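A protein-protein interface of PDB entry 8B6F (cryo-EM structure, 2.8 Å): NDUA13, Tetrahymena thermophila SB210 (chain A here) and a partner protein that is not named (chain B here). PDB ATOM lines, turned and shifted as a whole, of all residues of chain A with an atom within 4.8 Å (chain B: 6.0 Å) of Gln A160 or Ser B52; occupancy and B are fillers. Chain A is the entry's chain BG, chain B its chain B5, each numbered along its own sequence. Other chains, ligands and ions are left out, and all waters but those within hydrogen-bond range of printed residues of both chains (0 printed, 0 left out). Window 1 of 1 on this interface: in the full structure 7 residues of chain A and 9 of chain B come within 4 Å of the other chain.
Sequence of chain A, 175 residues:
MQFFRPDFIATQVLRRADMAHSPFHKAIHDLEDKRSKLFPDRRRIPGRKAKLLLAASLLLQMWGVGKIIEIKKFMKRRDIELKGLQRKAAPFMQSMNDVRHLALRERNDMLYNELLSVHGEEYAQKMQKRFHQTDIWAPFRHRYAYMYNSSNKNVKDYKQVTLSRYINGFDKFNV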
ATOM      1  N   LYS A 156     -23.927 -19.800 -12.414  1.00  0.00           N
ATOM      2  CA  LYS A 156     -24.820 -20.790 -11.826  1.00  0.00           C
ATOM      3  C   LYS A 156     -25.749 -20.067 -10.863  1.00  0.00           C
ATOM      4  O   LYS A 156     -25.593 -18.873 -10.604  1.00  0.00           O
ATOM      5  CB  LYS A 156     -24.053 -21.893 -11.089  1.00  0.00           C
ATOM      6  CG  LYS A 156     -23.260 -22.841 -11.977  1.00  0.00           C
ATOM      7  CD  LYS A 156     -22.779 -24.059 -11.207  1.00  0.00           C
ATOM      8  CE  LYS A 156     -21.855 -23.675 -10.065  1.00  0.00           C
ATOM      9  NZ  LYS A 156     -20.670 -22.901 -10.521  1.00  0.00           N
ATOM     10  N   ASP A 157     -26.728 -20.801 -10.350  1.00  0.00           N
ATOM     11  CA  ASP A 157     -27.541 -20.307  -9.251  1.00  0.00           C
ATOM     12  C   ASP A 157     -26.802 -20.507  -7.929  1.00  0.00           C
ATOM     13  O   ASP A 157     -25.806 -21.226  -7.848  1.00  0.00           O
ATOM     14  CB  ASP A 157     -28.894 -21.016  -9.219  1.00  0.00           C
ATOM     15  CG  ASP A 157     -29.694 -20.799 -10.488  1.00  0.00           C
ATOM     16  OD1 ASP A 157     -29.476 -19.771 -11.160  1.00  0.00           O
ATOM     17  OD2 ASP A 157     -30.544 -21.656 -10.812  1.00  0.00           O
ATOM     18  N   TYR A 158     -27.306 -19.863  -6.877  1.00  0.00           N
ATOM     19  CA  TYR A 158     -26.680 -20.018  -5.567  1.00  0.00           C
ATOM     20  C   TYR A 158     -26.773 -21.460  -5.088  1.00  0.00           C
ATOM     21  O   TYR A 158     -25.818 -21.993  -4.511  1.00  0.00           O
ATOM     22  CB  TYR A 158     -27.321 -19.065  -4.558  1.00  0.00           C
ATOM     23  CG  TYR A 158     -27.002 -17.615  -4.823  1.00  0.00           C
ATOM     24  CD1 TYR A 158     -25.799 -17.070  -4.401  1.00  0.00           C
ATOM     25  CD2 TYR A 158     -27.896 -16.793  -5.494  1.00  0.00           C
ATOM     26  CE1 TYR A 158     -25.492 -15.751  -4.636  1.00  0.00           C
ATOM     27  CE2 TYR A 158     -27.597 -15.466  -5.735  1.00  0.00           C
ATOM     28  CZ  TYR A 158     -26.390 -14.954  -5.302  1.00  0.00           C
ATOM     29  OH  TYR A 158     -26.069 -13.639  -5.528  1.00  0.00           O
ATOM     30  N   LYS A 159     -27.916 -22.106  -5.314  1.00  0.00           N
ATOM     31  CA  LYS A 159     -28.067 -23.503  -4.921  1.00  0.00           C
ATOM     32  C   LYS A 159     -27.052 -24.384  -5.637  1.00  0.00           C
ATOM     33  O   LYS A 159     -26.415 -25.244  -5.022  1.00  0.00           O
ATOM     34  CB  LYS A 159     -29.484 -23.972  -5.236  1.00  0.00           C
ATOM     35  CG  LYS A 159     -29.729 -25.446  -4.979  1.00  0.00           C
ATOM     36  CD  LYS A 159     -31.160 -25.777  -5.325  1.00  0.00           C
ATOM     37  CE  LYS A 159     -31.485 -27.238  -5.144  1.00  0.00           C
ATOM     38  NZ  LYS A 159     -32.916 -27.423  -5.507  1.00  0.00           N
ATOM     39  N   GLN A 160     -26.893 -24.185  -6.946  1.00  0.00           N
ATOM     40  CA  GLN A 160     -25.911 -24.959  -7.696  1.00  0.00           C
ATOM     41  C   GLN A 160     -24.499 -24.675  -7.207  1.00  0.00           C
ATOM     42  O   GLN A 160     -23.687 -25.595  -7.062  1.00  0.00           O
ATOM     43  CB  GLN A 160     -26.027 -24.654  -9.187  1.00  0.00           C
ATOM     44  CG  GLN A 160     -27.371 -25.016  -9.791  1.00  0.00           C
ATOM     45  CD  GLN A 160     -27.435 -24.715 -11.275  1.00  0.00           C
ATOM     46  OE1 GLN A 160     -28.407 -24.137 -11.759  1.00  0.00           O
ATOM     47  NE2 GLN A 160     -26.403 -25.115 -12.009  1.00  0.00           N
ATOM     48  N   VAL A 161     -24.185 -23.404  -6.954  1.00  0.00           N
ATOM     49  CA  VAL A 161     -22.852 -23.052  -6.476  1.00  0.00           C
ATOM     50  C   VAL A 161     -22.551 -23.773  -5.171  1.00  0.00           C
ATOM     51  O   VAL A 161     -21.441 -24.279  -4.968  1.00  0.00           O
ATOM     52  CB  VAL A 161     -22.738 -21.523  -6.319  1.00  0.00           C
ATOM     53  CG1 VAL A 161     -21.512 -21.143  -5.497  1.00  0.00           C
ATOM     54  CG2 VAL A 161     -22.680 -20.857  -7.681  1.00  0.00           C
ATOM     55  N   THR A 162     -23.525 -23.828  -4.264  1.00  0.00           N
ATOM     56  CA  THR A 162     -23.300 -24.497  -2.988  1.00  0.00           C
ATOM     57  C   THR A 162     -23.159 -26.004  -3.170  1.00  0.00           C
ATOM     58  O   THR A 162     -22.238 -26.621  -2.623  1.00  0.00           O
ATOM     59  CB  THR A 162     -24.447 -24.177  -2.027  1.00  0.00           C
ATOM     60  OG1 THR A 162     -24.542 -22.758  -1.846  1.00  0.00           O
ATOM     61  CG2 THR A 162     -24.219 -24.835  -0.675  1.00  0.00           C
ATOM     62  N   LEU A 163     -24.059 -26.613  -3.941  1.00  0.00           N
ATOM     63  CA  LEU A 163     -24.122 -28.070  -3.999  1.00  0.00           C
ATOM     64  C   LEU A 163     -23.017 -28.666  -4.859  1.00  0.00           C
ATOM     65  O   LEU A 163     -22.461 -29.714  -4.515  1.00  0.00           O
ATOM     66  CB  LEU A 163     -25.490 -28.515  -4.516  1.00  0.00           C
ATOM     67  CG  LEU A 163     -26.685 -28.237  -3.601  1.00  0.00           C
ATOM     68  CD1 LEU A 163     -27.970 -28.722  -4.252  1.00  0.00           C
ATOM     69  CD2 LEU A 163     -26.510 -28.878  -2.229  1.00  0.00           C
ATOM     70  N   SER A 164     -22.682 -28.025  -5.979  1.00  0.00           N
ATOM     71  CA  SER A 164     -21.765 -28.644  -6.928  1.00  0.00           C
ATOM     72  C   SER A 164     -20.392 -28.904  -6.325  1.00  0.00           C
ATOM     73  O   SER A 164     -19.632 -29.709  -6.872  1.00  0.00           O
ATOM     74  CB  SER A 164     -21.623 -27.765  -8.169  1.00  0.00           C
ATOM     75  OG  SER A 164     -21.199 -26.462  -7.820  1.00  0.00           O
ATOM     76  N   PHE A 170     -23.532 -31.880 -11.287  1.00  0.00           N
ATOM     77  CA  PHE A 170     -23.701 -30.472 -11.629  1.00  0.00           C
ATOM     78  C   PHE A 170     -22.711 -30.027 -12.698  1.00  0.00           C
ATOM     79  O   PHE A 170     -23.047 -29.198 -13.551  1.00  0.00           O
ATOM     80  CB  PHE A 170     -23.557 -29.610 -10.375  1.00  0.00           C
ATOM     81  CG  PHE A 170     -24.723 -29.714  -9.437  1.00  0.00           C
ATOM     82  CD1 PHE A 170     -24.831 -30.781  -8.562  1.00  0.00           C
ATOM     83  CD2 PHE A 170     -25.709 -28.743  -9.428  1.00  0.00           C
ATOM     84  CE1 PHE A 170     -25.903 -30.878  -7.697  1.00  0.00           C
ATOM     85  CE2 PHE A 170     -26.783 -28.834  -8.565  1.00  0.00           C
ATOM     86  CZ  PHE A 170     -26.879 -29.901  -7.698  1.00  0.00           C
ATOM     87  N   ASN B  48     -39.028 -25.285 -18.841  1.00  0.00           N
ATOM     88  CA  ASN B  48     -37.643 -24.855 -18.809  1.00  0.00           C
ATOM     89  C   ASN B  48     -36.846 -25.649 -19.832  1.00  0.00           C
ATOM     90  O   ASN B  48     -37.156 -26.817 -20.087  1.00  0.00           O
ATOM     91  CB  ASN B  48     -37.045 -25.057 -17.408  1.00  0.00           C
ATOM     92  CG  ASN B  48     -35.678 -24.427 -17.257  1.00  0.00           C
ATOM     93  OD1 ASN B  48     -34.656 -25.058 -17.523  1.00  0.00           O
ATOM     94  ND2 ASN B  48     -35.650 -23.173 -16.821  1.00  0.00           N
ATOM     95  N   PRO B  49     -35.821 -25.046 -20.443  1.00  0.00           N
ATOM     96  CA  PRO B  49     -34.976 -25.827 -21.361  1.00  0.00           C
ATOM     97  C   PRO B  49     -34.328 -27.027 -20.697  1.00  0.00           C
ATOM     98  O   PRO B  49     -34.118 -28.053 -21.355  1.00  0.00           O
ATOM     99  CB  PRO B  49     -33.932 -24.803 -21.832  1.00  0.00           C
ATOM    100  CG  PRO B  49     -34.588 -23.487 -21.656  1.00  0.00           C
ATOM    101  CD  PRO B  49     -35.456 -23.619 -20.443  1.00  0.00           C
ATOM    102  N   ARG B  50     -34.001 -26.927 -19.409  1.00  0.00           N
ATOM    103  CA  ARG B  50     -33.455 -28.042 -18.639  1.00  0.00           C
ATOM    104  C   ARG B  50     -32.128 -28.533 -19.208  1.00  0.00           C
ATOM    105  O   ARG B  50     -31.796 -29.716 -19.104  1.00  0.00           O
ATOM    106  CB  ARG B  50     -34.460 -29.195 -18.555  1.00  0.00           C
ATOM    107  CG  ARG B  50     -35.708 -28.844 -17.760  1.00  0.00           C
ATOM    108  CD  ARG B  50     -36.706 -29.990 -17.732  1.00  0.00           C
ATOM    109  NE  ARG B  50     -36.170 -31.180 -17.085  1.00  0.00           N
ATOM    110  CZ  ARG B  50     -36.884 -32.255 -16.782  1.00  0.00           C
ATOM    111  NH1 ARG B  50     -38.180 -32.318 -17.039  1.00  0.00           N
ATOM    112  NH2 ARG B  50     -36.286 -33.292 -16.205  1.00  0.00           N
ATOM    113  N   TYR B  51     -31.356 -27.631 -19.813  1.00  0.00           N
ATOM    114  CA  TYR B  51     -29.995 -27.953 -20.217  1.00  0.00           C
ATOM    115  C   TYR B  51     -29.002 -27.847 -19.069  1.00  0.00           C
ATOM    116  O   TYR B  51     -27.861 -28.297 -19.215  1.00  0.00           O
ATOM    117  CB  TYR B  51     -29.550 -27.033 -21.356  1.00  0.00           C
ATOM    118  CG  TYR B  51     -30.263 -27.284 -22.661  1.00  0.00           C
ATOM    119  CD1 TYR B  51     -30.152 -28.504 -23.313  1.00  0.00           C
ATOM    120  CD2 TYR B  51     -31.032 -26.292 -23.252  1.00  0.00           C
ATOM    121  CE1 TYR B  51     -30.798 -28.735 -24.510  1.00  0.00           C
ATOM    122  CE2 TYR B  51     -31.683 -26.513 -24.450  1.00  0.00           C
ATOM    123  CZ  TYR B  51     -31.561 -27.736 -25.073  1.00  0.00           C
ATOM    124  OH  TYR B  51     -32.207 -27.958 -26.267  1.00  0.00           O
ATOM    125  N   SER B  52     -29.406 -27.271 -17.941  1.00  0.00           N
ATOM    126  CA  SER B  52     -28.562 -27.132 -16.765  1.00  0.00           C
ATOM    127  C   SER B  52     -29.140 -27.959 -15.626  1.00  0.00           C
ATOM    128  O   SER B  52     -30.351 -27.946 -15.388  1.00  0.00           O
ATOM    129  CB  SER B  52     -28.449 -25.666 -16.341  1.00  0.00           C
ATOM    130  OG  SER B  52     -27.611 -25.532 -15.205  1.00  0.00           O
ATOM    131  N   TYR B  53     -28.268 -28.676 -14.924  1.00  0.00           N
ATOM    132  CA  TYR B  53     -28.688 -29.572 -13.850  1.00  0.00           C
ATOM    133  C   TYR B  53     -29.082 -28.739 -12.639  1.00  0.00           C
ATOM    134  O   TYR B  53     -28.235 -28.351 -11.834  1.00  0.00           O
ATOM    135  CB  TYR B  53     -27.567 -30.546 -13.512  1.00  0.00           C
ATOM    136  CG  TYR B  53     -28.018 -31.736 -12.703  1.00  0.00           C
ATOM    137  CD1 TYR B  53     -28.556 -32.853 -13.324  1.00  0.00           C
ATOM    138  CD2 TYR B  53     -27.899 -31.747 -11.321  1.00  0.00           C
ATOM    139  CE1 TYR B  53     -28.967 -33.945 -12.594  1.00  0.00           C
ATOM    140  CE2 TYR B  53     -28.308 -32.834 -10.582  1.00  0.00           C
ATOM    141  CZ  TYR B  53     -28.840 -33.930 -11.225  1.00  0.00           C
ATOM    142  OH  TYR B  53     -29.249 -35.015 -10.492  1.00  0.00           O
ATOM    143  N   THR B  54     -30.379 -28.464 -12.503  1.00  0.00           N
ATOM    144  CA  THR B  54     -30.891 -27.625 -11.429  1.00  0.00           C
ATOM    145  C   THR B  54     -31.716 -28.382 -10.402  1.00  0.00           C
ATOM    146  O   THR B  54     -31.693 -28.016  -9.226  1.00  0.00           O
ATOM    147  CB  THR B  54     -31.746 -26.488 -12.001  1.00  0.00           C
ATOM    148  OG1 THR B  54     -31.036 -25.833 -13.060  1.00  0.00           O
ATOM    149  CG2 THR B  54     -32.073 -25.469 -10.920  1.00  0.00           C
ATOM    150  N   MET B  55     -32.445 -29.419 -10.811  1.00  0.00           N
ATOM    151  CA  MET B  55     -33.256 -30.206  -9.886  1.00  0.00           C
ATOM    152  C   MET B  55     -32.679 -31.611  -9.778  1.00  0.00           C
ATOM    153  O   MET B  55     -32.907 -32.445 -10.667  1.00  0.00           O
ATOM    154  CB  MET B  55     -34.712 -30.263 -10.357  1.00  0.00           C
ATOM    155  CG  MET B  55     -35.420 -28.919 -10.355  1.00  0.00           C
ATOM    156  SD  MET B  55     -35.149 -27.961 -11.854  1.00  0.00           S
ATOM    157  CE  MET B  55     -36.127 -28.893 -13.024  1.00  0.00           C
ATOM    158  N   GLN B  59     -33.749 -34.477 -12.990  1.00  0.00           N
ATOM    159  CA  GLN B  59     -33.035 -34.440 -14.254  1.00  0.00           C
ATOM    160  C   GLN B  59     -31.989 -35.546 -14.282  1.00  0.00           C
ATOM    161  O   GLN B  59     -31.401 -35.898 -13.256  1.00  0.00           O
ATOM    162  CB  GLN B  59     -32.357 -33.084 -14.461  1.00  0.00           C
ATOM    163  CG  GLN B  59     -33.310 -31.903 -14.479  1.00  0.00           C
ATOM    164  CD  GLN B  59     -32.635 -30.626 -14.930  1.00  0.00           C
ATOM    165  OE1 GLN B  59     -31.491 -30.640 -15.378  1.00  0.00           O
ATOM    166  NE2 GLN B  59     -33.344 -29.510 -14.815  1.00  0.00           N
ATOM    167  N   LEU B  71     -31.380 -32.765 -19.845  1.00  0.00           N
ATOM    168  CA  LEU B  71     -31.149 -33.599 -18.673  1.00  0.00           C
ATOM    169  C   LEU B  71     -32.465 -33.942 -17.986  1.00  0.00           C
ATOM    170  O   LEU B  71     -33.448 -33.213 -18.109  1.00  0.00           O
ATOM    171  CB  LEU B  71     -30.212 -32.895 -17.690  1.00  0.00           C
ATOM    172  CG  LEU B  71     -28.832 -32.510 -18.232  1.00  0.00           C
ATOM    173  CD1 LEU B  71     -28.040 -31.756 -17.179  1.00  0.00           C
ATOM    174  CD2 LEU B  71     -28.064 -33.734 -18.701  1.00  0.00           C
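The side-chain amide nitrogen (NE2) of Gln A160 is in hydrogen-bond range of the side-chain hydroxyl (OG) of Ser B52 (3.4 Å).
The side-chain amide oxygen (OE1) of Gln A160 lies within hydrogen-bond range of the side-chain hydroxyl (OG1) of Thr B54, at 3.4 Å.
OG1 of Thr B54 lies within hydrogen-bond range of O of Ser B52, at 3.2 Å.
The backbone carbonyl oxygen (O) of Ser B52 lies close to the side-chain amide oxygen (OE1) of Gln B59, 2.9 Å away.
OD2 of Asp A157 sits close to OE1 of Gln A160.
The backbone carbonyl oxygen (O) of Gln A160 is in hydrogen-bond range of the side-chain hydroxyl (OG) of Ser A164, at 2.7 Å.
Among the printed residues, merely in contact across the chains: Lys A159 with Thr B54, Gln A160 with Tyr B53 and Phe A170 with Tyr B53.
Asp A157 touches none of the printed residues of chain B.
Of the printed residues of chain B, Lys A159 touches Thr B54.
Printed residues of chain B within 4 Å of Gln A160: Ser B52, Tyr B53 and Thr B54.
Leu A163 touches none of the printed residues of chain B.
Ser B52 touches just one residue of chain A: Gln A160 (3.4 Å).
Of the printed residues of chain A, Tyr B53 touches Gln A160 (3.7 Å) and Phe A170 (3.5 Å).
The nearest printed residue of chain A that does not touch Ser B52 is Lys A156 (6.0 Å).
Hydrophobic or aromatic side chains of chain A within 4 Å of the printed part of chain B: Phe A170.
Of the 10 printed residues of chain B, 3 touch a printed residue of chain A.
Among the printed residues, 5 pairs touch across the chains.
Among the printed residues, no Asp or Glu carboxylate lies within 4 Å of a Lys or Arg side-chain nitrogen of the other chain.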
